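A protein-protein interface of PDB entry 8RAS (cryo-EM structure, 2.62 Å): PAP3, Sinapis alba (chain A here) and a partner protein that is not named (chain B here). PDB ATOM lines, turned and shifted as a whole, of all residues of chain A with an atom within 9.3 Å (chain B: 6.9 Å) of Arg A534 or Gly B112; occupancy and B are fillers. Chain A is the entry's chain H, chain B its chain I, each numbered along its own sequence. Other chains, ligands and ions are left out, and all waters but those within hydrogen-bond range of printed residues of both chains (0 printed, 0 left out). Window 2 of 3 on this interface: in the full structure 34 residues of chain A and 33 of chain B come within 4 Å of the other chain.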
ATOM      1  N   ALA A 526     -38.293  16.280  15.279  1.00  0.00           N
ATOM      2  CA  ALA A 526     -37.547  15.451  14.341  1.00  0.00           C
ATOM      3  C   ALA A 526     -36.539  16.292  13.567  1.00  0.00           C
ATOM      4  O   ALA A 526     -35.421  15.844  13.290  1.00  0.00           O
ATOM      5  CB  ALA A 526     -38.508  14.739  13.391  1.00  0.00           C
ATOM      6  N   LEU A 527     -36.911  17.532  13.246  1.00  0.00           N
ATOM      7  CA  LEU A 527     -36.025  18.423  12.509  1.00  0.00           C
ATOM      8  C   LEU A 527     -34.776  18.758  13.314  1.00  0.00           C
ATOM      9  O   LEU A 527     -33.657  18.657  12.802  1.00  0.00           O
ATOM     10  CB  LEU A 527     -36.797  19.688  12.137  1.00  0.00           C
ATOM     11  CG  LEU A 527     -36.343  20.577  10.988  1.00  0.00           C
ATOM     12  CD1 LEU A 527     -37.556  20.902  10.165  1.00  0.00           C
ATOM     13  CD2 LEU A 527     -35.737  21.855  11.504  1.00  0.00           C
ATOM     14  N   LEU A 528     -34.949  19.150  14.579  1.00  0.00           N
ATOM     15  CA  LEU A 528     -33.799  19.466  15.425  1.00  0.00           C
ATOM     16  C   LEU A 528     -32.902  18.251  15.618  1.00  0.00           C
ATOM     17  O   LEU A 528     -31.669  18.377  15.624  1.00  0.00           O
ATOM     18  CB  LEU A 528     -34.253  20.017  16.779  1.00  0.00           C
ATOM     19  CG  LEU A 528     -34.581  21.508  16.927  1.00  0.00           C
ATOM     20  CD1 LEU A 528     -33.310  22.325  16.755  1.00  0.00           C
ATOM     21  CD2 LEU A 528     -35.649  21.988  15.962  1.00  0.00           C
ATOM     22  N   ARG A 529     -33.495  17.066  15.781  1.00  0.00           N
ATOM     23  CA  ARG A 529     -32.668  15.864  15.829  1.00  0.00           C
ATOM     24  C   ARG A 529     -31.902  15.669  14.524  1.00  0.00           C
ATOM     25  O   ARG A 529     -30.748  15.222  14.539  1.00  0.00           O
ATOM     26  CB  ARG A 529     -33.525  14.638  16.141  1.00  0.00           C
ATOM     27  CG  ARG A 529     -34.242  14.716  17.478  1.00  0.00           C
ATOM     28  CD  ARG A 529     -34.730  13.349  17.934  1.00  0.00           C
ATOM     29  NE  ARG A 529     -36.066  13.036  17.444  1.00  0.00           N
ATOM     30  CZ  ARG A 529     -36.368  11.959  16.731  1.00  0.00           C
ATOM     31  NH1 ARG A 529     -35.448  11.064  16.408  1.00  0.00           N
ATOM     32  NH2 ARG A 529     -37.624  11.771  16.337  1.00  0.00           N
ATOM     33  N   ASP A 530     -32.524  16.011  13.392  1.00  0.00           N
ATOM     34  CA  ASP A 530     -31.840  15.920  12.106  1.00  0.00           C
ATOM     35  C   ASP A 530     -30.648  16.871  12.042  1.00  0.00           C
ATOM     36  O   ASP A 530     -29.572  16.494  11.568  1.00  0.00           O
ATOM     37  CB  ASP A 530     -32.820  16.212  10.969  1.00  0.00           C
ATOM     38  CG  ASP A 530     -33.542  14.972  10.491  1.00  0.00           C
ATOM     39  OD1 ASP A 530     -32.868  14.022  10.041  1.00  0.00           O
ATOM     40  OD2 ASP A 530     -34.787  14.949  10.566  1.00  0.00           O
ATOM     41  N   ILE A 531     -30.826  18.115  12.497  1.00  0.00           N
ATOM     42  CA  ILE A 531     -29.694  19.044  12.537  1.00  0.00           C
ATOM     43  C   ILE A 531     -28.586  18.504  13.429  1.00  0.00           C
ATOM     44  O   ILE A 531     -27.403  18.543  13.062  1.00  0.00           O
ATOM     45  CB  ILE A 531     -30.114  20.468  12.968  1.00  0.00           C
ATOM     46  CG1 ILE A 531     -31.016  21.150  11.937  1.00  0.00           C
ATOM     47  CG2 ILE A 531     -28.908  21.328  13.309  1.00  0.00           C
ATOM     48  CD1 ILE A 531     -32.435  21.230  12.312  1.00  0.00           C
ATOM     49  N   SER A 532     -28.943  17.994  14.608  1.00  0.00           N
ATOM     50  CA  SER A 532     -27.926  17.450  15.505  1.00  0.00           C
ATOM     51  C   SER A 532     -27.129  16.349  14.817  1.00  0.00           C
ATOM     52  O   SER A 532     -25.893  16.403  14.759  1.00  0.00           O
ATOM     53  CB  SER A 532     -28.582  16.922  16.781  1.00  0.00           C
ATOM     54  OG  SER A 532     -29.010  15.583  16.615  1.00  0.00           O
ATOM     55  N   SER A 533     -27.827  15.366  14.242  1.00  0.00           N
ATOM     56  CA  SER A 533     -27.144  14.244  13.605  1.00  0.00           C
ATOM     57  C   SER A 533     -26.302  14.699  12.417  1.00  0.00           C
ATOM     58  O   SER A 533     -25.158  14.255  12.252  1.00  0.00           O
ATOM     59  CB  SER A 533     -28.166  13.195  13.167  1.00  0.00           C
ATOM     60  OG  SER A 533     -29.010  12.830  14.245  1.00  0.00           O
ATOM     61  N   ARG A 534     -26.842  15.591  11.582  1.00  0.00           N
ATOM     62  CA  ARG A 534     -26.150  15.972  10.355  1.00  0.00           C
ATOM     63  C   ARG A 534     -24.905  16.802  10.648  1.00  0.00           C
ATOM     64  O   ARG A 534     -23.834  16.541  10.089  1.00  0.00           O
ATOM     65  CB  ARG A 534     -27.106  16.720   9.425  1.00  0.00           C
ATOM     66  CG  ARG A 534     -28.166  15.820   8.803  1.00  0.00           C
ATOM     67  CD  ARG A 534     -29.186  16.611   8.002  1.00  0.00           C
ATOM     68  NE  ARG A 534     -30.227  15.751   7.449  1.00  0.00           N
ATOM     69  CZ  ARG A 534     -30.065  14.952   6.403  1.00  0.00           C
ATOM     70  NH1 ARG A 534     -28.909  14.871   5.766  1.00  0.00           N
ATOM     71  NH2 ARG A 534     -31.090  14.215   5.985  1.00  0.00           N
ATOM     72  N   GLN A 535     -25.018  17.808  11.519  1.00  0.00           N
ATOM     73  CA  GLN A 535     -23.827  18.548  11.921  1.00  0.00           C
ATOM     74  C   GLN A 535     -22.859  17.702  12.733  1.00  0.00           C
ATOM     75  O   GLN A 535     -21.673  18.041  12.801  1.00  0.00           O
ATOM     76  CB  GLN A 535     -24.215  19.806  12.696  1.00  0.00           C
ATOM     77  CG  GLN A 535     -24.263  21.062  11.840  1.00  0.00           C
ATOM     78  CD  GLN A 535     -25.668  21.497  11.517  1.00  0.00           C
ATOM     79  OE1 GLN A 535     -26.583  20.680  11.484  1.00  0.00           O
ATOM     80  NE2 GLN A 535     -25.853  22.792  11.294  1.00  0.00           N
ATOM     81  N   ALA A 536     -23.324  16.614  13.349  1.00  0.00           N
ATOM     82  CA  ALA A 536     -22.380  15.680  13.947  1.00  0.00           C
ATOM     83  C   ALA A 536     -21.681  14.827  12.896  1.00  0.00           C
ATOM     84  O   ALA A 536     -20.566  14.351  13.134  1.00  0.00           O
ATOM     85  CB  ALA A 536     -23.094  14.787  14.960  1.00  0.00           C
ATOM     86  N   LEU A 537     -22.312  14.624  11.739  1.00  0.00           N
ATOM     87  CA  LEU A 537     -21.766  13.749  10.711  1.00  0.00           C
ATOM     88  C   LEU A 537     -21.477  14.449   9.389  1.00  0.00           C
ATOM     89  O   LEU A 537     -21.066  13.782   8.433  1.00  0.00           O
ATOM     90  CB  LEU A 537     -22.717  12.570  10.470  1.00  0.00           C
ATOM     91  CG  LEU A 537     -22.861  11.638  11.673  1.00  0.00           C
ATOM     92  CD1 LEU A 537     -24.130  10.816  11.569  1.00  0.00           C
ATOM     93  CD2 LEU A 537     -21.643  10.741  11.806  1.00  0.00           C
ATOM     94  N   GLY A 538     -21.679  15.762   9.298  1.00  0.00           N
ATOM     95  CA  GLY A 538     -21.313  16.498   8.105  1.00  0.00           C
ATOM     96  C   GLY A 538     -22.258  16.367   6.933  1.00  0.00           C
ATOM     97  O   GLY A 538     -21.933  16.851   5.843  1.00  0.00           O
ATOM     98  N   LEU A 539     -23.412  15.729   7.112  1.00  0.00           N
ATOM     99  CA  LEU A 539     -24.364  15.602   6.023  1.00  0.00           C
ATOM    100  C   LEU A 539     -24.975  16.964   5.687  1.00  0.00           C
ATOM    101  O   LEU A 539     -25.063  17.843   6.548  1.00  0.00           O
ATOM    102  CB  LEU A 539     -25.468  14.614   6.392  1.00  0.00           C
ATOM    103  CG  LEU A 539     -25.159  13.135   6.162  1.00  0.00           C
ATOM    104  CD1 LEU A 539     -26.127  12.269   6.941  1.00  0.00           C
ATOM    105  CD2 LEU A 539     -25.209  12.798   4.683  1.00  0.00           C
ATOM    106  N   PRO A 540     -25.390  17.166   4.438  1.00  0.00           N
ATOM    107  CA  PRO A 540     -25.995  18.450   4.066  1.00  0.00           C
ATOM    108  C   PRO A 540     -27.311  18.687   4.789  1.00  0.00           C
ATOM    109  O   PRO A 540     -28.067  17.758   5.082  1.00  0.00           O
ATOM    110  CB  PRO A 540     -26.211  18.315   2.554  1.00  0.00           C
ATOM    111  CG  PRO A 540     -26.282  16.847   2.316  1.00  0.00           C
ATOM    112  CD  PRO A 540     -25.319  16.243   3.293  1.00  0.00           C
ATOM    113  N   LEU A 541     -27.577  19.961   5.074  1.00  0.00           N
ATOM    114  CA  LEU A 541     -28.809  20.360   5.748  1.00  0.00           C
ATOM    115  C   LEU A 541     -29.949  20.544   4.751  1.00  0.00           C
ATOM    116  O   LEU A 541     -30.999  19.906   4.871  1.00  0.00           O
ATOM    117  CB  LEU A 541     -28.575  21.647   6.544  1.00  0.00           C
ATOM    118  CG  LEU A 541     -27.724  21.504   7.805  1.00  0.00           C
ATOM    119  CD1 LEU A 541     -27.437  22.867   8.406  1.00  0.00           C
ATOM    120  CD2 LEU A 541     -28.412  20.596   8.811  1.00  0.00           C
ATOM    121  N   GLU A 542     -29.755  21.415   3.768  1.00  0.00           N
ATOM    122  CA  GLU A 542     -30.724  21.608   2.703  1.00  0.00           C
ATOM    123  C   GLU A 542     -30.331  20.781   1.483  1.00  0.00           C
ATOM    124  O   GLU A 542     -29.227  20.238   1.394  1.00  0.00           O
ATOM    125  CB  GLU A 542     -30.837  23.090   2.345  1.00  0.00           C
ATOM    126  CG  GLU A 542     -30.746  24.020   3.543  1.00  0.00           C
ATOM    127  CD  GLU A 542     -31.821  25.088   3.542  1.00  0.00           C
ATOM    128  OE1 GLU A 542     -31.618  26.137   4.189  1.00  0.00           O
ATOM    129  OE2 GLU A 542     -32.868  24.880   2.893  1.00  0.00           O
ATOM    130  N   GLU A 543     -31.255  20.684   0.535  1.00  0.00           N
ATOM    131  CA  GLU A 543     -31.027  19.859  -0.642  1.00  0.00           C
ATOM    132  C   GLU A 543     -29.887  20.436  -1.475  1.00  0.00           C
ATOM    133  O   GLU A 543     -29.916  21.627  -1.817  1.00  0.00           O
ATOM    134  CB  GLU A 543     -32.297  19.764  -1.483  1.00  0.00           C
ATOM    135  CG  GLU A 543     -32.200  18.782  -2.635  1.00  0.00           C
ATOM    136  CD  GLU A 543     -33.484  18.694  -3.432  1.00  0.00           C
ATOM    137  OE1 GLU A 543     -34.135  19.740  -3.630  1.00  0.00           O
ATOM    138  OE2 GLU A 543     -33.844  17.576  -3.859  1.00  0.00           O
ATOM    139  N   PRO A 544     -28.869  19.643  -1.809  1.00  0.00           N
ATOM    140  CA  PRO A 544     -27.779  20.155  -2.647  1.00  0.00           C
ATOM    141  C   PRO A 544     -28.280  20.544  -4.029  1.00  0.00           C
ATOM    142  O   PRO A 544     -29.222  19.954  -4.563  1.00  0.00           O
ATOM    143  CB  PRO A 544     -26.798  18.978  -2.716  1.00  0.00           C
ATOM    144  CG  PRO A 544     -27.153  18.107  -1.552  1.00  0.00           C
ATOM    145  CD  PRO A 544     -28.629  18.258  -1.373  1.00  0.00           C
ATOM    146  N   TYR B 109     -26.849   6.995  -1.917  1.00  0.00           N
ATOM    147  CA  TYR B 109     -26.589   8.216  -1.162  1.00  0.00           C
ATOM    148  C   TYR B 109     -27.782   9.163  -1.227  1.00  0.00           C
ATOM    149  O   TYR B 109     -28.092   9.847  -0.245  1.00  0.00           O
ATOM    150  CB  TYR B 109     -25.326   8.899  -1.683  1.00  0.00           C
ATOM    151  CG  TYR B 109     -24.970  10.163  -0.937  1.00  0.00           C
ATOM    152  CD1 TYR B 109     -24.667  10.126   0.417  1.00  0.00           C
ATOM    153  CD2 TYR B 109     -24.935  11.390  -1.583  1.00  0.00           C
ATOM    154  CE1 TYR B 109     -24.341  11.273   1.107  1.00  0.00           C
ATOM    155  CE2 TYR B 109     -24.608  12.545  -0.901  1.00  0.00           C
ATOM    156  CZ  TYR B 109     -24.314  12.480   0.444  1.00  0.00           C
ATOM    157  OH  TYR B 109     -23.991  13.627   1.132  1.00  0.00           O
ATOM    158  N   ASN B 110     -28.452   9.218  -2.379  1.00  0.00           N
ATOM    159  CA  ASN B 110     -29.713   9.944  -2.540  1.00  0.00           C
ATOM    160  C   ASN B 110     -29.565  11.425  -2.197  1.00  0.00           C
ATOM    161  O   ASN B 110     -30.423  12.017  -1.538  1.00  0.00           O
ATOM    162  CB  ASN B 110     -30.823   9.296  -1.707  1.00  0.00           C
ATOM    163  CG  ASN B 110     -32.210   9.725  -2.142  1.00  0.00           C
ATOM    164  OD1 ASN B 110     -32.371  10.442  -3.127  1.00  0.00           O
ATOM    165  ND2 ASN B 110     -33.221   9.285  -1.403  1.00  0.00           N
ATOM    166  N   ASN B 111     -28.464  12.026  -2.650  1.00  0.00           N
ATOM    167  CA  ASN B 111     -28.238  13.469  -2.536  1.00  0.00           C
ATOM    168  C   ASN B 111     -28.334  13.946  -1.086  1.00  0.00           C
ATOM    169  O   ASN B 111     -29.030  14.913  -0.769  1.00  0.00           O
ATOM    170  CB  ASN B 111     -29.207  14.241  -3.432  1.00  0.00           C
ATOM    171  CG  ASN B 111     -28.636  15.560  -3.908  1.00  0.00           C
ATOM    172  OD1 ASN B 111     -27.420  15.731  -3.983  1.00  0.00           O
ATOM    173  ND2 ASN B 111     -29.513  16.502  -4.233  1.00  0.00           N
ATOM    174  N   GLY B 112     -27.624  13.256  -0.200  1.00  0.00           N
ATOM    175  CA  GLY B 112     -27.581  13.630   1.197  1.00  0.00           C
ATOM    176  C   GLY B 112     -28.687  13.067   2.058  1.00  0.00           C
ATOM    177  O   GLY B 112     -28.783  13.440   3.234  1.00  0.00           O
ATOM    178  N   ASN B 113     -29.521  12.183   1.519  1.00  0.00           N
ATOM    179  CA  ASN B 113     -30.587  11.522   2.271  1.00  0.00           C
ATOM    180  C   ASN B 113     -30.446  10.019   2.059  1.00  0.00           C
ATOM    181  O   ASN B 113     -31.258   9.395   1.366  1.00  0.00           O
ATOM    182  CB  ASN B 113     -31.961  12.025   1.830  1.00  0.00           C
ATOM    183  CG  ASN B 113     -33.081  11.504   2.703  1.00  0.00           C
ATOM    184  OD1 ASN B 113     -32.856  11.077   3.835  1.00  0.00           O
ATOM    185  ND2 ASN B 113     -34.301  11.535   2.180  1.00  0.00           N
ATOM    186  N   PRO B 114     -29.424   9.408   2.658  1.00  0.00           N
ATOM    187  CA  PRO B 114     -29.039   8.044   2.268  1.00  0.00           C
ATOM    188  C   PRO B 114     -30.158   7.031   2.456  1.00  0.00           C
ATOM    189  O   PRO B 114     -30.914   7.078   3.429  1.00  0.00           O
ATOM    190  CB  PRO B 114     -27.852   7.738   3.188  1.00  0.00           C
ATOM    191  CG  PRO B 114     -27.317   9.072   3.575  1.00  0.00           C
ATOM    192  CD  PRO B 114     -28.512   9.969   3.667  1.00  0.00           C
ATOM    193  N   SER B 194     -16.719  11.297   7.455  1.00  0.00           N
ATOM    194  CA  SER B 194     -17.248  10.576   8.601  1.00  0.00           C
ATOM    195  C   SER B 194     -18.159   9.437   8.160  1.00  0.00           C
ATOM    196  O   SER B 194     -18.784   9.491   7.096  1.00  0.00           O
ATOM    197  CB  SER B 194     -18.022  11.518   9.528  1.00  0.00           C
ATOM    198  OG  SER B 194     -19.390  11.577   9.160  1.00  0.00           O
ATOM    199  N   TRP B 202     -19.185  12.555  -4.447  1.00  0.00           N
ATOM    200  CA  TRP B 202     -18.820  13.840  -5.028  1.00  0.00           C
ATOM    201  C   TRP B 202     -18.216  13.695  -6.417  1.00  0.00           C
ATOM    202  O   TRP B 202     -17.679  14.672  -6.952  1.00  0.00           O
ATOM    203  CB  TRP B 202     -17.839  14.583  -4.117  1.00  0.00           C
ATOM    204  CG  TRP B 202     -18.080  14.423  -2.643  1.00  0.00           C
ATOM    205  CD1 TRP B 202     -17.137  14.178  -1.687  1.00  0.00           C
ATOM    206  CD2 TRP B 202     -19.329  14.557  -1.947  1.00  0.00           C
ATOM    207  NE1 TRP B 202     -17.722  14.115  -0.447  1.00  0.00           N
ATOM    208  CE2 TRP B 202     -19.066  14.347  -0.578  1.00  0.00           C
ATOM    209  CE3 TRP B 202     -20.643  14.818  -2.349  1.00  0.00           C
ATOM    210  CZ2 TRP B 202     -20.067  14.391   0.388  1.00  0.00           C
ATOM    211  CZ3 TRP B 202     -21.636  14.859  -1.387  1.00  0.00           C
ATOM    212  CH2 TRP B 202     -21.342  14.648  -0.035  1.00  0.00           C
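Arg A534 touches just one residue of chain B: Gly B112.
Gly B112 touches just these residues of chain A: Arg A534, Leu A539 and Pro A540.
Printed residues of chain B within 4 Å of Pro A540: Tyr B109 (3.6 Å) and Gly B112 (3.6 Å).
Printed residues of chain B within 4 Å of Pro A544: Asn B111.
Asp A530 touches none of the printed residues of chain B.
The nearest residue of chain A that does not touch Gly B112 is Pro A544 (5.1 Å).
Of the 8 printed residues of chain B, 4 touch a printed residue of chain A.
Printed residues of chain B that touch a printed residue of chain A: Tyr B109, Asn B111, Gly B112 and Ser B194.
Of the 19 printed residues of chain A, 6 touch a printed residue of chain B.
Along chain A the printed residues that touch a printed residue of chain B span positions 534 to 544.
Among the printed residues, merely in contact across the chains: Pro A540 with Tyr B109, Pro A540 with Gly B112, Leu A539 with Tyr B109, Glu A543 with Asn B111 and Leu A539 with Gly B112.
NH1 of Arg A534 is in hydrogen-bond range of O of Gly B112, 2.9 Å away.
O of Leu A537 lies within hydrogen-bond range of OG of Ser B194 (2.9 Å).
ND2 of Asn B111 sits close to O of Pro A544, at 3.5 Å.
The guanidinium group (NH1) of Arg A534 is in hydrogen-bond range of the backbone carbonyl oxygen (O) of Pro A540 (3.1 Å).
N of Leu A539 sits at hydrogen-bond distance from O of Arg A534, at 3.1 Å.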
